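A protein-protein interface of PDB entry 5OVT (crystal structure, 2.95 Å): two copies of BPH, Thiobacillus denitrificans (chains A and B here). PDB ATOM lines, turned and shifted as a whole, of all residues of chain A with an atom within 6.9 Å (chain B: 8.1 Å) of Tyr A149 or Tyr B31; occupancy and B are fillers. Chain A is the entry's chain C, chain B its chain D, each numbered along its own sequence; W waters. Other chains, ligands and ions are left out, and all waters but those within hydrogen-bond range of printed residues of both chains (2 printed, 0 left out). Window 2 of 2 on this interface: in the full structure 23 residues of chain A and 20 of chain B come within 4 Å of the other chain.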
ATOM      1  N   ILE A 119       4.259   9.213 -25.068  1.00  0.00           N
ATOM      2  CA  ILE A 119       3.626  10.509 -25.413  1.00  0.00           C
ATOM      3  C   ILE A 119       3.711  10.815 -26.893  1.00  0.00           C
ATOM      4  O   ILE A 119       4.732  10.655 -27.531  1.00  0.00           O
ATOM      5  CB  ILE A 119       4.200  11.711 -24.633  1.00  0.00           C
ATOM      6  CG1 ILE A 119       5.712  11.822 -24.802  1.00  0.00           C
ATOM      7  CG2 ILE A 119       3.870  11.556 -23.162  1.00  0.00           C
ATOM      8  CD1 ILE A 119       6.255  13.112 -24.243  1.00  0.00           C
ATOM      9  N   GLU A 130       6.018  10.409 -32.072  1.00  0.00           N
ATOM     10  CA  GLU A 130       6.239  10.073 -30.707  1.00  0.00           C
ATOM     11  C   GLU A 130       7.285  11.040 -30.188  1.00  0.00           C
ATOM     12  O   GLU A 130       8.314  11.217 -30.824  1.00  0.00           O
ATOM     13  CB  GLU A 130       6.668   8.614 -30.516  1.00  0.00           C
ATOM     14  CG  GLU A 130       6.878   8.362 -29.037  1.00  0.00           C
ATOM     15  CD  GLU A 130       7.179   6.929 -28.626  1.00  0.00           C
ATOM     16  OE1 GLU A 130       7.390   6.086 -29.496  1.00  0.00           O
ATOM     17  OE2 GLU A 130       7.241   6.696 -27.392  1.00  0.00           O
ATOM     18  N   PHE A 131       7.041  11.624 -29.014  1.00  0.00           N
ATOM     19  CA  PHE A 131       7.966  12.561 -28.406  1.00  0.00           C
ATOM     20  C   PHE A 131       8.812  11.939 -27.291  1.00  0.00           C
ATOM     21  O   PHE A 131       8.347  11.076 -26.540  1.00  0.00           O
ATOM     22  CB  PHE A 131       7.223  13.737 -27.817  1.00  0.00           C
ATOM     23  CG  PHE A 131       6.420  14.472 -28.798  1.00  0.00           C
ATOM     24  CD1 PHE A 131       7.002  15.161 -29.791  1.00  0.00           C
ATOM     25  CD2 PHE A 131       5.057  14.450 -28.733  1.00  0.00           C
ATOM     26  CE1 PHE A 131       6.241  15.810 -30.750  1.00  0.00           C
ATOM     27  CE2 PHE A 131       4.272  15.103 -29.676  1.00  0.00           C
ATOM     28  CZ  PHE A 131       4.880  15.786 -30.681  1.00  0.00           C
ATOM     29  N   SER A 132      10.033  12.431 -27.153  1.00  0.00           N
ATOM     30  CA  SER A 132      10.974  11.831 -26.253  1.00  0.00           C
ATOM     31  C   SER A 132      11.144  12.623 -24.962  1.00  0.00           C
ATOM     32  O   SER A 132      11.412  12.029 -23.957  1.00  0.00           O
ATOM     33  CB  SER A 132      12.294  11.618 -26.939  1.00  0.00           C
ATOM     34  OG  SER A 132      12.879  12.881 -27.155  1.00  0.00           O
ATOM     35  N   LYS A 133      10.859  13.920 -24.947  1.00  0.00           N
ATOM     36  CA  LYS A 133      10.866  14.683 -23.690  1.00  0.00           C
ATOM     37  C   LYS A 133       9.591  15.521 -23.453  1.00  0.00           C
ATOM     38  O   LYS A 133       8.837  15.298 -22.502  1.00  0.00           O
ATOM     39  CB  LYS A 133      12.024  15.623 -23.695  1.00  0.00           C
ATOM     40  CG  LYS A 133      13.385  15.046 -24.021  1.00  0.00           C
ATOM     41  CD  LYS A 133      14.305  16.235 -24.378  1.00  0.00           C
ATOM     42  CE  LYS A 133      15.753  15.883 -24.565  1.00  0.00           C
ATOM     43  NZ  LYS A 133      15.840  14.596 -25.323  1.00  0.00           N
ATOM     44  N   PHE A 134       9.363  16.499 -24.309  1.00  0.00           N
ATOM     45  CA  PHE A 134       8.133  17.264 -24.243  1.00  0.00           C
ATOM     46  C   PHE A 134       7.788  17.886 -25.577  1.00  0.00           C
ATOM     47  O   PHE A 134       8.635  17.996 -26.468  1.00  0.00           O
ATOM     48  CB  PHE A 134       8.250  18.392 -23.235  1.00  0.00           C
ATOM     49  CG  PHE A 134       9.334  19.381 -23.551  1.00  0.00           C
ATOM     50  CD1 PHE A 134       9.125  20.385 -24.444  1.00  0.00           C
ATOM     51  CD2 PHE A 134      10.575  19.312 -22.910  1.00  0.00           C
ATOM     52  CE1 PHE A 134      10.146  21.288 -24.735  1.00  0.00           C
ATOM     53  CE2 PHE A 134      11.583  20.206 -23.174  1.00  0.00           C
ATOM     54  CZ  PHE A 134      11.370  21.202 -24.096  1.00  0.00           C
ATOM     55  N   TYR A 135       6.534  18.301 -25.700  1.00  0.00           N
ATOM     56  CA  TYR A 135       6.101  19.047 -26.853  1.00  0.00           C
ATOM     57  C   TYR A 135       4.819  19.817 -26.580  1.00  0.00           C
ATOM     58  O   TYR A 135       4.242  19.699 -25.512  1.00  0.00           O
ATOM     59  CB  TYR A 135       5.981  18.168 -28.107  1.00  0.00           C
ATOM     60  CG  TYR A 135       6.332  19.006 -29.320  1.00  0.00           C
ATOM     61  CD1 TYR A 135       7.618  19.507 -29.472  1.00  0.00           C
ATOM     62  CD2 TYR A 135       5.344  19.386 -30.261  1.00  0.00           C
ATOM     63  CE1 TYR A 135       7.948  20.330 -30.526  1.00  0.00           C
ATOM     64  CE2 TYR A 135       5.660  20.207 -31.313  1.00  0.00           C
ATOM     65  CZ  TYR A 135       6.967  20.688 -31.443  1.00  0.00           C
ATOM     66  OH  TYR A 135       7.283  21.493 -32.492  1.00  0.00           O
ATOM     67  N   TYR A 143       5.468  29.583 -26.957  1.00  0.00           N
ATOM     68  CA  TYR A 143       5.727  30.143 -25.643  1.00  0.00           C
ATOM     69  C   TYR A 143       5.913  28.959 -24.725  1.00  0.00           C
ATOM     70  O   TYR A 143       6.800  28.931 -23.876  1.00  0.00           O
ATOM     71  CB  TYR A 143       4.567  31.004 -25.146  1.00  0.00           C
ATOM     72  CG  TYR A 143       4.181  32.143 -26.069  1.00  0.00           C
ATOM     73  CD1 TYR A 143       4.749  33.417 -25.949  1.00  0.00           C
ATOM     74  CD2 TYR A 143       3.211  31.958 -27.050  1.00  0.00           C
ATOM     75  CE1 TYR A 143       4.378  34.466 -26.784  1.00  0.00           C
ATOM     76  CE2 TYR A 143       2.839  33.015 -27.877  1.00  0.00           C
ATOM     77  CZ  TYR A 143       3.440  34.254 -27.745  1.00  0.00           C
ATOM     78  OH  TYR A 143       2.996  35.236 -28.550  1.00  0.00           O
ATOM     79  N   ALA A 144       5.048  27.969 -24.881  1.00  0.00           N
ATOM     80  CA  ALA A 144       5.119  26.798 -24.019  1.00  0.00           C
ATOM     81  C   ALA A 144       6.414  26.021 -24.222  1.00  0.00           C
ATOM     82  O   ALA A 144       7.003  25.558 -23.273  1.00  0.00           O
ATOM     83  CB  ALA A 144       3.917  25.910 -24.286  1.00  0.00           C
ATOM     84  N   LEU A 145       6.865  25.913 -25.462  1.00  0.00           N
ATOM     85  CA  LEU A 145       8.086  25.194 -25.746  1.00  0.00           C
ATOM     86  C   LEU A 145       9.267  25.866 -25.064  1.00  0.00           C
ATOM     87  O   LEU A 145      10.139  25.193 -24.537  1.00  0.00           O
ATOM     88  CB  LEU A 145       8.362  25.082 -27.253  1.00  0.00           C
ATOM     89  CG  LEU A 145       7.445  24.142 -28.031  1.00  0.00           C
ATOM     90  CD1 LEU A 145       7.735  24.233 -29.509  1.00  0.00           C
ATOM     91  CD2 LEU A 145       7.622  22.698 -27.571  1.00  0.00           C
ATOM     92  N   GLY A 146       9.297  27.190 -25.094  1.00  0.00           N
ATOM     93  CA  GLY A 146      10.408  27.911 -24.495  1.00  0.00           C
ATOM     94  C   GLY A 146      10.450  27.705 -22.987  1.00  0.00           C
ATOM     95  O   GLY A 146      11.498  27.428 -22.415  1.00  0.00           O
ATOM     96  N   ALA A 147       9.301  27.871 -22.356  1.00  0.00           N
ATOM     97  CA  ALA A 147       9.215  27.698 -20.955  1.00  0.00           C
ATOM     98  C   ALA A 147       9.671  26.272 -20.566  1.00  0.00           C
ATOM     99  O   ALA A 147      10.379  26.078 -19.581  1.00  0.00           O
ATOM    100  CB  ALA A 147       7.790  27.965 -20.501  1.00  0.00           C
ATOM    101  N   MET A 148       9.213  25.275 -21.309  1.00  0.00           N
ATOM    102  CA  MET A 148       9.521  23.892 -20.942  1.00  0.00           C
ATOM    103  C   MET A 148      10.975  23.613 -21.220  1.00  0.00           C
ATOM    104  O   MET A 148      11.616  22.845 -20.515  1.00  0.00           O
ATOM    105  CB  MET A 148       8.559  22.890 -21.624  1.00  0.00           C
ATOM    106  CG  MET A 148       7.138  23.118 -21.077  1.00  0.00           C
ATOM    107  SD  MET A 148       5.853  21.783 -21.731  1.00  0.00           S
ATOM    108  CE  MET A 148       5.921  22.247 -23.653  1.00  0.00           C
ATOM    109  N   TYR A 149      11.510  24.193 -22.272  1.00  0.00           N
ATOM    110  CA  TYR A 149      12.933  24.067 -22.512  1.00  0.00           C
ATOM    111  C   TYR A 149      13.689  24.576 -21.294  1.00  0.00           C
ATOM    112  O   TYR A 149      14.598  23.967 -20.890  1.00  0.00           O
ATOM    113  CB  TYR A 149      13.335  24.854 -23.767  1.00  0.00           C
ATOM    114  CG  TYR A 149      14.798  25.025 -23.977  1.00  0.00           C
ATOM    115  CD1 TYR A 149      15.582  24.034 -24.584  1.00  0.00           C
ATOM    116  CD2 TYR A 149      15.414  26.191 -23.585  1.00  0.00           C
ATOM    117  CE1 TYR A 149      16.965  24.213 -24.772  1.00  0.00           C
ATOM    118  CE2 TYR A 149      16.772  26.382 -23.778  1.00  0.00           C
ATOM    119  CZ  TYR A 149      17.525  25.390 -24.363  1.00  0.00           C
ATOM    120  OH  TYR A 149      18.831  25.659 -24.492  1.00  0.00           O
ATOM    121  N   ALA A 150      13.286  25.681 -20.706  1.00  0.00           N
ATOM    122  CA  ALA A 150      14.013  26.220 -19.595  1.00  0.00           C
ATOM    123  C   ALA A 150      13.870  25.382 -18.361  1.00  0.00           C
ATOM    124  O   ALA A 150      14.735  25.360 -17.552  1.00  0.00           O
ATOM    125  CB  ALA A 150      13.528  27.642 -19.292  1.00  0.00           C
ATOM    126  N   ALA A 151      12.734  24.742 -18.179  1.00  0.00           N
ATOM    127  CA  ALA A 151      12.410  24.079 -16.907  1.00  0.00           C
ATOM    128  C   ALA A 151      12.598  22.578 -16.923  1.00  0.00           C
ATOM    129  O   ALA A 151      12.538  21.956 -15.875  1.00  0.00           O
ATOM    130  CB  ALA A 151      10.962  24.378 -16.531  1.00  0.00           C
ATOM    131  N   TYR A 152      12.746  21.966 -18.092  1.00  0.00           N
ATOM    132  CA  TYR A 152      12.702  20.499 -18.173  1.00  0.00           C
ATOM    133  C   TYR A 152      13.731  19.784 -17.327  1.00  0.00           C
ATOM    134  O   TYR A 152      13.411  18.762 -16.714  1.00  0.00           O
ATOM    135  CB  TYR A 152      12.865  20.057 -19.590  1.00  0.00           C
ATOM    136  CG  TYR A 152      12.722  18.586 -19.769  1.00  0.00           C
ATOM    137  CD1 TYR A 152      11.495  17.969 -19.603  1.00  0.00           C
ATOM    138  CD2 TYR A 152      13.793  17.807 -20.136  1.00  0.00           C
ATOM    139  CE1 TYR A 152      11.339  16.598 -19.777  1.00  0.00           C
ATOM    140  CE2 TYR A 152      13.637  16.446 -20.341  1.00  0.00           C
ATOM    141  CZ  TYR A 152      12.418  15.853 -20.126  1.00  0.00           C
ATOM    142  OH  TYR A 152      12.266  14.539 -20.311  1.00  0.00           O
ATOM    143  N   ARG A 153      14.940  20.349 -17.222  1.00  0.00           N
ATOM    144  CA  ARG A 153      16.015  19.725 -16.398  1.00  0.00           C
ATOM    145  C   ARG A 153      16.052  20.233 -14.967  1.00  0.00           C
ATOM    146  O   ARG A 153      16.830  19.770 -14.203  1.00  0.00           O
ATOM    147  CB  ARG A 153      17.364  19.878 -17.044  1.00  0.00           C
ATOM    148  CG  ARG A 153      17.280  19.417 -18.462  1.00  0.00           C
ATOM    149  CD  ARG A 153      18.571  19.010 -19.137  1.00  0.00           C
ATOM    150  NE  ARG A 153      18.351  17.618 -19.600  1.00  0.00           N
ATOM    151  CZ  ARG A 153      18.055  17.200 -20.843  1.00  0.00           C
ATOM    152  NH1 ARG A 153      17.972  18.033 -21.908  1.00  0.00           N
ATOM    153  NH2 ARG A 153      17.857  15.899 -21.040  1.00  0.00           N
ATOM    154  N   VAL A 162       6.032  20.808 -15.247  1.00  0.00           N
ATOM    155  CA  VAL A 162       6.597  21.309 -16.477  1.00  0.00           C
ATOM    156  C   VAL A 162       5.502  21.496 -17.516  1.00  0.00           C
ATOM    157  O   VAL A 162       5.445  22.501 -18.203  1.00  0.00           O
ATOM    158  CB  VAL A 162       7.666  20.345 -17.016  1.00  0.00           C
ATOM    159  CG1 VAL A 162       8.092  20.707 -18.421  1.00  0.00           C
ATOM    160  CG2 VAL A 162       8.900  20.360 -16.119  1.00  0.00           C
ATOM    161  N   THR B  18      17.461  14.111 -40.264  1.00  0.00           N
ATOM    162  CA  THR B  18      16.496  13.684 -39.211  1.00  0.00           C
ATOM    163  C   THR B  18      15.648  14.808 -38.665  1.00  0.00           C
ATOM    164  O   THR B  18      15.008  14.658 -37.633  1.00  0.00           O
ATOM    165  CB  THR B  18      17.237  13.033 -38.013  1.00  0.00           C
ATOM    166  OG1 THR B  18      18.214  13.953 -37.464  1.00  0.00           O
ATOM    167  CG2 THR B  18      17.886  11.734 -38.474  1.00  0.00           C
ATOM    168  N   LYS B  26      11.242  23.849 -35.561  1.00  0.00           N
ATOM    169  CA  LYS B  26      12.120  22.728 -35.737  1.00  0.00           C
ATOM    170  C   LYS B  26      11.826  21.676 -34.717  1.00  0.00           C
ATOM    171  O   LYS B  26      11.824  21.976 -33.542  1.00  0.00           O
ATOM    172  CB  LYS B  26      13.537  23.165 -35.472  1.00  0.00           C
ATOM    173  CG  LYS B  26      14.068  24.150 -36.469  1.00  0.00           C
ATOM    174  CD  LYS B  26      15.556  24.308 -36.348  1.00  0.00           C
ATOM    175  CE  LYS B  26      15.860  24.932 -35.019  1.00  0.00           C
ATOM    176  NZ  LYS B  26      17.208  25.484 -35.172  1.00  0.00           N
ATOM    177  N   GLU B  27      11.643  20.445 -35.183  1.00  0.00           N
ATOM    178  CA  GLU B  27      11.450  19.295 -34.346  1.00  0.00           C
ATOM    179  C   GLU B  27      12.610  18.381 -34.590  1.00  0.00           C
ATOM    180  O   GLU B  27      12.566  17.522 -35.497  1.00  0.00           O
ATOM    181  CB  GLU B  27      10.131  18.614 -34.696  1.00  0.00           C
ATOM    182  CG  GLU B  27       8.883  19.354 -34.189  1.00  0.00           C
ATOM    183  CD  GLU B  27       7.572  18.929 -34.859  1.00  0.00           C
ATOM    184  OE1 GLU B  27       6.602  18.535 -34.152  1.00  0.00           O
ATOM    185  OE2 GLU B  27       7.482  18.966 -36.104  1.00  0.00           O
ATOM    186  N   SER B  28      13.695  18.596 -33.823  1.00  0.00           N
ATOM    187  CA  SER B  28      14.949  17.819 -34.042  1.00  0.00           C
ATOM    188  C   SER B  28      14.824  16.368 -33.531  1.00  0.00           C
ATOM    189  O   SER B  28      13.862  16.034 -32.866  1.00  0.00           O
ATOM    190  CB  SER B  28      16.115  18.507 -33.368  1.00  0.00           C
ATOM    191  OG  SER B  28      16.221  18.152 -32.001  1.00  0.00           O
ATOM    192  N   ALA B  29      15.765  15.499 -33.867  1.00  0.00           N
ATOM    193  CA  ALA B  29      15.769  14.091 -33.385  1.00  0.00           C
ATOM    194  C   ALA B  29      15.891  13.963 -31.891  1.00  0.00           C
ATOM    195  O   ALA B  29      15.540  12.960 -31.319  1.00  0.00           O
ATOM    196  CB  ALA B  29      16.891  13.312 -34.023  1.00  0.00           C
ATOM    197  N   ASP B  30      16.345  15.016 -31.255  1.00  0.00           N
ATOM    198  CA  ASP B  30      16.457  15.082 -29.836  1.00  0.00           C
ATOM    199  C   ASP B  30      15.035  15.182 -29.194  1.00  0.00           C
ATOM    200  O   ASP B  30      14.846  14.755 -28.075  1.00  0.00           O
ATOM    201  CB  ASP B  30      17.352  16.271 -29.598  1.00  0.00           C
ATOM    202  CG  ASP B  30      17.738  16.469 -28.196  1.00  0.00           C
ATOM    203  OD1 ASP B  30      17.871  15.510 -27.444  1.00  0.00           O
ATOM    204  OD2 ASP B  30      17.945  17.648 -27.813  1.00  0.00           O
ATOM    205  N   TYR B  31      14.009  15.671 -29.907  1.00  0.00           N
ATOM    206  CA  TYR B  31      12.607  15.778 -29.372  1.00  0.00           C
ATOM    207  C   TYR B  31      11.646  14.792 -29.980  1.00  0.00           C
ATOM    208  O   TYR B  31      10.611  14.470 -29.375  1.00  0.00           O
ATOM    209  CB  TYR B  31      12.034  17.193 -29.576  1.00  0.00           C
ATOM    210  CG  TYR B  31      12.785  18.217 -28.789  1.00  0.00           C
ATOM    211  CD1 TYR B  31      12.402  18.540 -27.503  1.00  0.00           C
ATOM    212  CD2 TYR B  31      13.949  18.766 -29.285  1.00  0.00           C
ATOM    213  CE1 TYR B  31      13.154  19.422 -26.731  1.00  0.00           C
ATOM    214  CE2 TYR B  31      14.697  19.646 -28.541  1.00  0.00           C
ATOM    215  CZ  TYR B  31      14.288  19.991 -27.277  1.00  0.00           C
ATOM    216  OH  TYR B  31      15.036  20.904 -26.568  1.00  0.00           O
ATOM    217  N   VAL B  32      11.974  14.281 -31.159  1.00  0.00           N
ATOM    218  CA  VAL B  32      11.085  13.334 -31.808  1.00  0.00           C
ATOM    219  C   VAL B  32      11.697  11.988 -31.914  1.00  0.00           C
ATOM    220  O   VAL B  32      12.765  11.813 -32.514  1.00  0.00           O
ATOM    221  CB  VAL B  32      10.754  13.768 -33.241  1.00  0.00           C
ATOM    222  CG1 VAL B  32       9.927  12.703 -33.943  1.00  0.00           C
ATOM    223  CG2 VAL B  32       9.999  15.082 -33.226  1.00  0.00           C
ATOM    224  N   ALA B  33      11.051  11.024 -31.293  1.00  0.00           N
ATOM    225  CA  ALA B  33      11.613   9.655 -31.199  1.00  0.00           C
ATOM    226  C   ALA B  33      11.631   9.001 -32.529  1.00  0.00           C
ATOM    227  O   ALA B  33      12.591   8.393 -32.897  1.00  0.00           O
ATOM    228  CB  ALA B  33      10.779   8.807 -30.243  1.00  0.00           C
ATOM    229  N   ASN B  34      10.543   9.132 -33.252  1.00  0.00           N
ATOM    230  CA  ASN B  34      10.430   8.484 -34.573  1.00  0.00           C
ATOM    231  C   ASN B  34      10.799   9.425 -35.737  1.00  0.00           C
ATOM    232  O   ASN B  34       9.970   9.686 -36.640  1.00  0.00           O
ATOM    233  CB  ASN B  34       9.039   7.921 -34.752  1.00  0.00           C
ATOM    234  CG  ASN B  34       7.966   8.995 -34.787  1.00  0.00           C
ATOM    235  OD1 ASN B  34       7.942   9.951 -34.008  1.00  0.00           O
ATOM    236  ND2 ASN B  34       7.018   8.779 -35.627  1.00  0.00           N
ATOM    237  N   HIS B  35      12.067   9.845 -35.709  1.00  0.00           N
ATOM    238  CA  HIS B  35      12.598  10.816 -36.605  1.00  0.00           C
ATOM    239  C   HIS B  35      13.196  10.207 -37.868  1.00  0.00           C
ATOM    240  O   HIS B  35      13.698  10.932 -38.698  1.00  0.00           O
ATOM    241  CB  HIS B  35      13.650  11.628 -35.890  1.00  0.00           C
ATOM    242  CG  HIS B  35      14.687  10.798 -35.205  1.00  0.00           C
ATOM    243  ND1 HIS B  35      14.708  10.625 -33.838  1.00  0.00           N
ATOM    244  CD2 HIS B  35      15.741  10.106 -35.684  1.00  0.00           C
ATOM    245  CE1 HIS B  35      15.714   9.833 -33.507  1.00  0.00           C
ATOM    246  NE2 HIS B  35      16.352   9.495 -34.613  1.00  0.00           N
HETATM  247  O   HOH W   1      10.075  15.665 -26.990  1.00  0.00           O
HETATM  248  O   HOH W   2       9.355  23.293 -32.648  1.00  0.00           O
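OD1 of Asn B34 sits at hydrogen-bond distance from N of Glu A130 (2.8 Å).
The backbone carbonyl oxygen (O) of Asp B30 lies within hydrogen-bond range of the side-chain hydroxyl (OG) of Ser A132.
OH of Tyr A135 sits close to OE1 of Glu B27 (3.5 Å).
The side-chain amino group (NZ) of Lys A133 lies within salt-bridge range of the side-chain carboxylate (OD1) of Asp B30, 3.1 Å away.
The backbone NH of Ser A132 lies within hydrogen-bond range of the backbone carbonyl oxygen of Tyr B31 (3.1 Å).
O of Glu A130 lies within hydrogen-bond range of N of Ala B33, 2.8 Å away.
O of Ala B33 is in hydrogen-bond range of ND1 of His B35, 3.2 Å away.
The backbone carbonyl oxygen (O) of Val B32 sits at hydrogen-bond distance from a ring nitrogen (ND1) of His B35 (2.6 Å).
The backbone carbonyl oxygen (O) of Ile A119 lies within hydrogen-bond range of the backbone NH (N) of Phe A131 (2.9 Å).
OG of Ser B28 sits close to N of Asp B30 (3.2 Å).
Among the printed residues, pairs that only touch across the chains: Glu A130 with Val B32 (3.6 Å), Phe A131 with Tyr B31 (3.4 Å), Phe A134 with Tyr B31 (3.6 Å) and Tyr A149 with Tyr B31 (3.7 Å).
Tyr B31 touches four residues of chain A.
No residue of chain B comes within 4 Å of Ala A150.
Printed residues of chain B within 4 Å of Ser A132: Asp B30 (2.9 Å) and Tyr B31 (3.1 Å).
Of the printed residues of chain B, Tyr A135 touches Glu B27.
Of the printed residues of chain A, Asp B30 touches Ser A132 and Lys A133.
Printed residues of chain A within 4 Å of Asn B34: Glu A130 (2.8 Å).
Printed residues of chain A within 4 Å of Val B32: Glu A130 (3.6 Å).
Ala A147 touches none of the printed residues of chain B.
Arg A153 touches none of the printed residues of chain B.
The nearest residue of chain B that does not touch Tyr A149 is Asp B30 (7.3 Å).
Printed residues of chain B that touch a printed residue of chain A: Glu B27, Asp B30, Tyr B31, Val B32, Ala B33 and Asn B34.
Hydrophobic or aromatic side chains of chain B within 4 Å of the printed part of chain A: Tyr B31, Val B32 and Ala B33.
Hydrophobic or aromatic side chains of chain A within 4 Å of the printed part of chain B: Phe A131, Phe A134, Tyr A135 and Tyr A149.
Among the printed residues, 10 pairs touch across the chains.
Among the printed residues, Asp or Glu carboxylates within 4 Å of a Lys or Arg side-chain nitrogen of the other chain: Lys A133 with Asp B30 (3.1 Å).
No position is printed for both chains.
Of the 10 pairs that touch across the chains among the printed residues, none has its exchanged pair printed and touching as well.
Water W1 lies within hydrogen-bond range of O of Tyr B31 (2.7 Å), O of Phe A134 (2.8 Å), N of Lys A133 (2.8 Å) and N of Ser A132 (3.2 Å).
Water W2 lies within hydrogen-bond range of OH of Tyr A135 (2.7 Å) and O of Lys B26 (2.9 Å).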
